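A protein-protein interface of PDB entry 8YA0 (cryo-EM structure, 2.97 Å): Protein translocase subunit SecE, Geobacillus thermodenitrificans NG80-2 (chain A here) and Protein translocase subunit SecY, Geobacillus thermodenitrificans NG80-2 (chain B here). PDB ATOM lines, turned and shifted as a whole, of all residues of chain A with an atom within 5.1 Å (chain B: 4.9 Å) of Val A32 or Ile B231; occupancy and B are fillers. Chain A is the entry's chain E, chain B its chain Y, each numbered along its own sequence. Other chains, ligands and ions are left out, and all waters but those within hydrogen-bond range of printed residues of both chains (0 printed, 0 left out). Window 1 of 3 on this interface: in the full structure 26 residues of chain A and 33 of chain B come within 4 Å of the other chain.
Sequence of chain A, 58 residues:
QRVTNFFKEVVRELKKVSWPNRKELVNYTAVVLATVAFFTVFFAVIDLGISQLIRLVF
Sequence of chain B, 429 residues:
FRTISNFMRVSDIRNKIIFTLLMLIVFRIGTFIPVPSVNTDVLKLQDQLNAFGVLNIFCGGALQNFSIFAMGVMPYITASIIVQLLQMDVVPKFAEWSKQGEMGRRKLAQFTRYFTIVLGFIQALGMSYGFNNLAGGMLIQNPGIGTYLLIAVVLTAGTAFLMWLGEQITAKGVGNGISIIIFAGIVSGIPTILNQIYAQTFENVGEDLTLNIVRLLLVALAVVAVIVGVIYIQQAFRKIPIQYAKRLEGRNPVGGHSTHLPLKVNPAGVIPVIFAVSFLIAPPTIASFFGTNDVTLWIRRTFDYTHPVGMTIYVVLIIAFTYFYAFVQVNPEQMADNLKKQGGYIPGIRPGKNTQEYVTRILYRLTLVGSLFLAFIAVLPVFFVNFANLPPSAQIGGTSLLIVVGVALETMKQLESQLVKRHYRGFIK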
ATOM      1  N   PRO A  20     -18.568   7.921   9.985  1.00  0.00           N
ATOM      2  CA  PRO A  20     -19.921   8.008   9.433  1.00  0.00           C
ATOM      3  C   PRO A  20     -20.468   9.426   9.491  1.00  0.00           C
ATOM      4  O   PRO A  20     -20.258  10.160  10.457  1.00  0.00           O
ATOM      5  CB  PRO A  20     -20.726   7.049  10.315  1.00  0.00           C
ATOM      6  CG  PRO A  20     -19.950   6.899  11.518  1.00  0.00           C
ATOM      7  CD  PRO A  20     -18.527   7.028  11.147  1.00  0.00           C
ATOM      8  N   LEU A  25     -25.422   8.305  10.789  1.00  0.00           N
ATOM      9  CA  LEU A  25     -25.313   8.255  12.242  1.00  0.00           C
ATOM     10  C   LEU A  25     -26.682   8.288  12.898  1.00  0.00           C
ATOM     11  O   LEU A  25     -26.951   7.517  13.826  1.00  0.00           O
ATOM     12  CB  LEU A  25     -24.469   9.413  12.742  1.00  0.00           C
ATOM     13  CG  LEU A  25     -23.810   9.231  14.088  1.00  0.00           C
ATOM     14  CD1 LEU A  25     -22.822   8.143  13.965  1.00  0.00           C
ATOM     15  CD2 LEU A  25     -23.118  10.497  14.476  1.00  0.00           C
ATOM     16  N   TYR A  28     -28.480   4.967  12.127  1.00  0.00           N
ATOM     17  CA  TYR A  28     -27.931   3.881  12.928  1.00  0.00           C
ATOM     18  C   TYR A  28     -28.390   3.958  14.368  1.00  0.00           C
ATOM     19  O   TYR A  28     -28.718   2.930  14.962  1.00  0.00           O
ATOM     20  CB  TYR A  28     -26.413   3.910  12.884  1.00  0.00           C
ATOM     21  CG  TYR A  28     -25.812   3.387  11.626  1.00  0.00           C
ATOM     22  CD1 TYR A  28     -26.537   2.578  10.787  1.00  0.00           C
ATOM     23  CD2 TYR A  28     -24.520   3.710  11.276  1.00  0.00           C
ATOM     24  CE1 TYR A  28     -25.998   2.102   9.641  1.00  0.00           C
ATOM     25  CE2 TYR A  28     -23.971   3.241  10.129  1.00  0.00           C
ATOM     26  CZ  TYR A  28     -24.717   2.438   9.314  1.00  0.00           C
ATOM     27  OH  TYR A  28     -24.175   1.956   8.155  1.00  0.00           O
ATOM     28  N   THR A  29     -28.397   5.155  14.957  1.00  0.00           N
ATOM     29  CA  THR A  29     -28.878   5.284  16.326  1.00  0.00           C
ATOM     30  C   THR A  29     -30.358   4.973  16.431  1.00  0.00           C
ATOM     31  O   THR A  29     -30.798   4.403  17.430  1.00  0.00           O
ATOM     32  CB  THR A  29     -28.594   6.676  16.853  1.00  0.00           C
ATOM     33  OG1 THR A  29     -27.261   7.028  16.506  1.00  0.00           O
ATOM     34  CG2 THR A  29     -28.708   6.707  18.334  1.00  0.00           C
ATOM     35  N   ALA A  30     -31.127   5.287  15.391  1.00  0.00           N
ATOM     36  CA  ALA A  30     -32.532   4.917  15.366  1.00  0.00           C
ATOM     37  C   ALA A  30     -32.707   3.410  15.335  1.00  0.00           C
ATOM     38  O   ALA A  30     -33.551   2.871  16.051  1.00  0.00           O
ATOM     39  CB  ALA A  30     -33.213   5.548  14.162  1.00  0.00           C
ATOM     40  N   VAL A  31     -31.903   2.715  14.531  1.00  0.00           N
ATOM     41  CA  VAL A  31     -31.990   1.258  14.464  1.00  0.00           C
ATOM     42  C   VAL A  31     -31.576   0.627  15.789  1.00  0.00           C
ATOM     43  O   VAL A  31     -32.226  -0.305  16.273  1.00  0.00           O
ATOM     44  CB  VAL A  31     -31.147   0.735  13.292  1.00  0.00           C
ATOM     45  CG1 VAL A  31     -30.958  -0.746  13.372  1.00  0.00           C
ATOM     46  CG2 VAL A  31     -31.811   1.075  12.006  1.00  0.00           C
ATOM     47  N   VAL A  32     -30.540   1.168  16.431  1.00  0.00           N
ATOM     48  CA  VAL A  32     -30.047   0.594  17.679  1.00  0.00           C
ATOM     49  C   VAL A  32     -31.050   0.806  18.803  1.00  0.00           C
ATOM     50  O   VAL A  32     -31.385  -0.134  19.531  1.00  0.00           O
ATOM     51  CB  VAL A  32     -28.669   1.175  18.029  1.00  0.00           C
ATOM     52  CG1 VAL A  32     -28.359   1.006  19.483  1.00  0.00           C
ATOM     53  CG2 VAL A  32     -27.627   0.510  17.223  1.00  0.00           C
ATOM     54  N   LEU A  33     -31.579   2.022  18.938  1.00  0.00           N
ATOM     55  CA  LEU A  33     -32.562   2.272  19.983  1.00  0.00           C
ATOM     56  C   LEU A  33     -33.877   1.558  19.721  1.00  0.00           C
ATOM     57  O   LEU A  33     -34.515   1.102  20.669  1.00  0.00           O
ATOM     58  CB  LEU A  33     -32.796   3.763  20.141  1.00  0.00           C
ATOM     59  CG  LEU A  33     -31.614   4.509  20.733  1.00  0.00           C
ATOM     60  CD1 LEU A  33     -31.964   5.945  20.961  1.00  0.00           C
ATOM     61  CD2 LEU A  33     -31.189   3.878  22.019  1.00  0.00           C
ATOM     62  N   ALA A  34     -34.270   1.396  18.458  1.00  0.00           N
ATOM     63  CA  ALA A  34     -35.467   0.628  18.154  1.00  0.00           C
ATOM     64  C   ALA A  34     -35.284  -0.842  18.478  1.00  0.00           C
ATOM     65  O   ALA A  34     -36.196  -1.474  19.010  1.00  0.00           O
ATOM     66  CB  ALA A  34     -35.834   0.794  16.688  1.00  0.00           C
ATOM     67  N   THR A  35     -34.103  -1.396  18.199  1.00  0.00           N
ATOM     68  CA  THR A  35     -33.859  -2.802  18.494  1.00  0.00           C
ATOM     69  C   THR A  35     -33.799  -3.054  19.990  1.00  0.00           C
ATOM     70  O   THR A  35     -34.377  -4.029  20.478  1.00  0.00           O
ATOM     71  CB  THR A  35     -32.570  -3.249  17.830  1.00  0.00           C
ATOM     72  OG1 THR A  35     -32.452  -2.594  16.571  1.00  0.00           O
ATOM     73  CG2 THR A  35     -32.608  -4.713  17.581  1.00  0.00           C
ATOM     74  N   VAL A  36     -33.155  -2.162  20.735  1.00  0.00           N
ATOM     75  CA  VAL A  36     -33.053  -2.330  22.176  1.00  0.00           C
ATOM     76  C   VAL A  36     -34.406  -2.144  22.842  1.00  0.00           C
ATOM     77  O   VAL A  36     -34.774  -2.918  23.730  1.00  0.00           O
ATOM     78  CB  VAL A  36     -31.998  -1.369  22.735  1.00  0.00           C
ATOM     79  CG1 VAL A  36     -32.039  -1.318  24.228  1.00  0.00           C
ATOM     80  CG2 VAL A  36     -30.656  -1.815  22.294  1.00  0.00           C
ATOM     81  N   ALA A  37     -35.200  -1.169  22.389  1.00  0.00           N
ATOM     82  CA  ALA A  37     -36.517  -0.956  22.982  1.00  0.00           C
ATOM     83  C   ALA A  37     -37.484  -2.077  22.636  1.00  0.00           C
ATOM     84  O   ALA A  37     -38.236  -2.536  23.505  1.00  0.00           O
ATOM     85  CB  ALA A  37     -37.081   0.381  22.532  1.00  0.00           C
ATOM     86  N   ILE B 227     -24.189   5.730  23.224  1.00  0.00           N
ATOM     87  CA  ILE B 227     -24.560   4.867  22.104  1.00  0.00           C
ATOM     88  C   ILE B 227     -24.181   5.514  20.778  1.00  0.00           C
ATOM     89  O   ILE B 227     -23.696   4.841  19.862  1.00  0.00           O
ATOM     90  CB  ILE B 227     -26.057   4.531  22.180  1.00  0.00           C
ATOM     91  CG1 ILE B 227     -26.280   3.452  23.215  1.00  0.00           C
ATOM     92  CG2 ILE B 227     -26.602   4.053  20.868  1.00  0.00           C
ATOM     93  CD1 ILE B 227     -27.710   3.129  23.424  1.00  0.00           C
ATOM     94  N   VAL B 228     -24.331   6.833  20.676  1.00  0.00           N
ATOM     95  CA  VAL B 228     -23.903   7.544  19.471  1.00  0.00           C
ATOM     96  C   VAL B 228     -22.386   7.501  19.320  1.00  0.00           C
ATOM     97  O   VAL B 228     -21.871   7.271  18.223  1.00  0.00           O
ATOM     98  CB  VAL B 228     -24.439   8.982  19.495  1.00  0.00           C
ATOM     99  CG1 VAL B 228     -23.765   9.833  18.462  1.00  0.00           C
ATOM    100  CG2 VAL B 228     -25.901   8.971  19.240  1.00  0.00           C
ATOM    101  N   GLY B 229     -21.650   7.666  20.418  1.00  0.00           N
ATOM    102  CA  GLY B 229     -20.199   7.559  20.342  1.00  0.00           C
ATOM    103  C   GLY B 229     -19.713   6.166  19.987  1.00  0.00           C
ATOM    104  O   GLY B 229     -18.723   6.007  19.270  1.00  0.00           O
ATOM    105  N   VAL B 230     -20.422   5.143  20.449  1.00  0.00           N
ATOM    106  CA  VAL B 230     -20.054   3.770  20.143  1.00  0.00           C
ATOM    107  C   VAL B 230     -20.319   3.461  18.680  1.00  0.00           C
ATOM    108  O   VAL B 230     -19.499   2.824  18.020  1.00  0.00           O
ATOM    109  CB  VAL B 230     -20.795   2.815  21.093  1.00  0.00           C
ATOM    110  CG1 VAL B 230     -20.820   1.423  20.581  1.00  0.00           C
ATOM    111  CG2 VAL B 230     -20.133   2.819  22.410  1.00  0.00           C
ATOM    112  N   ILE B 231     -21.443   3.935  18.140  1.00  0.00           N
ATOM    113  CA  ILE B 231     -21.732   3.776  16.714  1.00  0.00           C
ATOM    114  C   ILE B 231     -20.719   4.528  15.873  1.00  0.00           C
ATOM    115  O   ILE B 231     -20.300   4.060  14.811  1.00  0.00           O
ATOM    116  CB  ILE B 231     -23.167   4.239  16.426  1.00  0.00           C
ATOM    117  CG1 ILE B 231     -24.149   3.264  17.015  1.00  0.00           C
ATOM    118  CG2 ILE B 231     -23.445   4.335  14.978  1.00  0.00           C
ATOM    119  CD1 ILE B 231     -25.503   3.776  17.039  1.00  0.00           C
ATOM    120  N   TYR B 232     -20.269   5.678  16.358  1.00  0.00           N
ATOM    121  CA  TYR B 232     -19.289   6.473  15.636  1.00  0.00           C
ATOM    122  C   TYR B 232     -17.944   5.766  15.538  1.00  0.00           C
ATOM    123  O   TYR B 232     -17.348   5.703  14.463  1.00  0.00           O
ATOM    124  CB  TYR B 232     -19.144   7.817  16.327  1.00  0.00           C
ATOM    125  CG  TYR B 232     -18.614   8.906  15.466  1.00  0.00           C
ATOM    126  CD1 TYR B 232     -19.273   9.282  14.322  1.00  0.00           C
ATOM    127  CD2 TYR B 232     -17.462   9.575  15.810  1.00  0.00           C
ATOM    128  CE1 TYR B 232     -18.791  10.279  13.537  1.00  0.00           C
ATOM    129  CE2 TYR B 232     -16.973  10.575  15.034  1.00  0.00           C
ATOM    130  CZ  TYR B 232     -17.642  10.923  13.899  1.00  0.00           C
ATOM    131  OH  TYR B 232     -17.153  11.935  13.113  1.00  0.00           O
ATOM    132  N   ILE B 233     -17.448   5.218  16.644  1.00  0.00           N
ATOM    133  CA  ILE B 233     -16.157   4.537  16.588  1.00  0.00           C
ATOM    134  C   ILE B 233     -16.280   3.185  15.904  1.00  0.00           C
ATOM    135  O   ILE B 233     -15.392   2.774  15.157  1.00  0.00           O
ATOM    136  CB  ILE B 233     -15.567   4.408  17.995  1.00  0.00           C
ATOM    137  CG1 ILE B 233     -15.332   5.780  18.576  1.00  0.00           C
ATOM    138  CG2 ILE B 233     -14.262   3.671  17.986  1.00  0.00           C
ATOM    139  CD1 ILE B 233     -14.306   6.549  17.858  1.00  0.00           C
ATOM    140  N   GLN B 234     -17.388   2.489  16.100  1.00  0.00           N
ATOM    141  CA  GLN B 234     -17.504   1.137  15.590  1.00  0.00           C
ATOM    142  C   GLN B 234     -17.682   1.073  14.089  1.00  0.00           C
ATOM    143  O   GLN B 234     -17.367   0.047  13.492  1.00  0.00           O
ATOM    144  CB  GLN B 234     -18.671   0.437  16.244  1.00  0.00           C
ATOM    145  CG  GLN B 234     -18.335  -0.233  17.523  1.00  0.00           C
ATOM    146  CD  GLN B 234     -19.312  -1.319  17.820  1.00  0.00           C
ATOM    147  OE1 GLN B 234     -20.172  -1.618  17.002  1.00  0.00           O
ATOM    148  NE2 GLN B 234     -19.195  -1.923  18.982  1.00  0.00           N
ATOM    149  N   GLN B 235     -18.176   2.129  13.461  1.00  0.00           N
ATOM    150  CA  GLN B 235     -18.488   2.097  12.043  1.00  0.00           C
ATOM    151  C   GLN B 235     -17.465   2.840  11.212  1.00  0.00           C
ATOM    152  O   GLN B 235     -17.724   3.150  10.054  1.00  0.00           O
ATOM    153  CB  GLN B 235     -19.868   2.678  11.800  1.00  0.00           C
ATOM    154  CG  GLN B 235     -20.965   1.905  12.424  1.00  0.00           C
ATOM    155  CD  GLN B 235     -21.189   0.620  11.733  1.00  0.00           C
ATOM    156  OE1 GLN B 235     -21.303   0.580  10.523  1.00  0.00           O
ATOM    157  NE2 GLN B 235     -21.259  -0.451  12.487  1.00  0.00           N
ATOM    158  N   VAL B 405     -24.747  -2.922  20.557  1.00  0.00           N
ATOM    159  CA  VAL B 405     -24.697  -2.050  19.386  1.00  0.00           C
ATOM    160  C   VAL B 405     -24.193  -2.806  18.167  1.00  0.00           C
ATOM    161  O   VAL B 405     -24.769  -2.702  17.078  1.00  0.00           O
ATOM    162  CB  VAL B 405     -23.829  -0.820  19.691  1.00  0.00           C
ATOM    163  CG1 VAL B 405     -23.520  -0.078  18.455  1.00  0.00           C
ATOM    164  CG2 VAL B 405     -24.526   0.079  20.649  1.00  0.00           C
ATOM    165  N   ALA B 408     -26.886  -5.403  16.913  1.00  0.00           N
ATOM    166  CA  ALA B 408     -28.019  -4.712  16.311  1.00  0.00           C
ATOM    167  C   ALA B 408     -27.686  -4.197  14.920  1.00  0.00           C
ATOM    168  O   ALA B 408     -28.432  -4.445  13.964  1.00  0.00           O
ATOM    169  CB  ALA B 408     -28.461  -3.565  17.205  1.00  0.00           C
ATOM    170  N   LEU B 409     -26.535  -3.538  14.772  1.00  0.00           N
ATOM    171  CA  LEU B 409     -26.165  -2.994  13.470  1.00  0.00           C
ATOM    172  C   LEU B 409     -25.822  -4.081  12.465  1.00  0.00           C
ATOM    173  O   LEU B 409     -26.159  -3.958  11.285  1.00  0.00           O
ATOM    174  CB  LEU B 409     -25.002  -2.036  13.615  1.00  0.00           C
ATOM    175  CG  LEU B 409     -25.330  -0.758  14.354  1.00  0.00           C
ATOM    176  CD1 LEU B 409     -24.167   0.156  14.292  1.00  0.00           C
ATOM    177  CD2 LEU B 409     -26.505  -0.117  13.725  1.00  0.00           C
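OG1 of Thr A29 sits at hydrogen-bond distance from O of Leu A25, 2.7 Å away.
Tyr B232 touches Pro A20.
Ile B231 touches Leu A25.
Leu A25 touches Tyr B232.
Gln B235 touches Tyr A28.
CD2 of Leu B409 touches O of Tyr A28, 3.96 Å away.
Val B228 touches Thr A29 (CG2 to OG1, 3.6 Å).
Thr A29 touches Ile B231.
CG1 of Val A32 touches CG2 of Ile B227 (3.8 Å).
CG2 of Val A32 touches CD1 of Ile B231, at 3.9 Å.
Ile B227 touches Leu A33.
Of the 12 printed residues of chain B, 6 touch a printed residue of chain A.
Printed residues of chain B that touch a printed residue of chain A: Ile B227, Val B228, Ile B231, Tyr B232, Gln B235 and Leu B409.
Among the printed residues, 12 pairs touch across the chains.
Among the printed residues, no Asp or Glu carboxylate lies within 4 Å of a Lys or Arg side-chain nitrogen of the other chain.
Of the printed residues of chain B, Leu A25 touches Ile B231 and Tyr B232.
Printed residues of chain A within 4 Å of Ile B227: Val A32 and Leu A33.
Of the printed residues of chain B, Tyr A28 touches Ile B231 (3.7 Å), Gln B235 (3.8 Å) and Leu B409 (3.96 Å).
Val A31 touches none of the printed residues of chain B.
The nearest residue of chain B that does not touch Val A32 is Val B405 (4.1 Å).
The nearest printed residue of chain A that does not touch Ile B231 is Pro A20 (4.4 Å).
The nearest printed residue of chain A that does not touch Val B228 is Leu A25 (4.1 Å).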
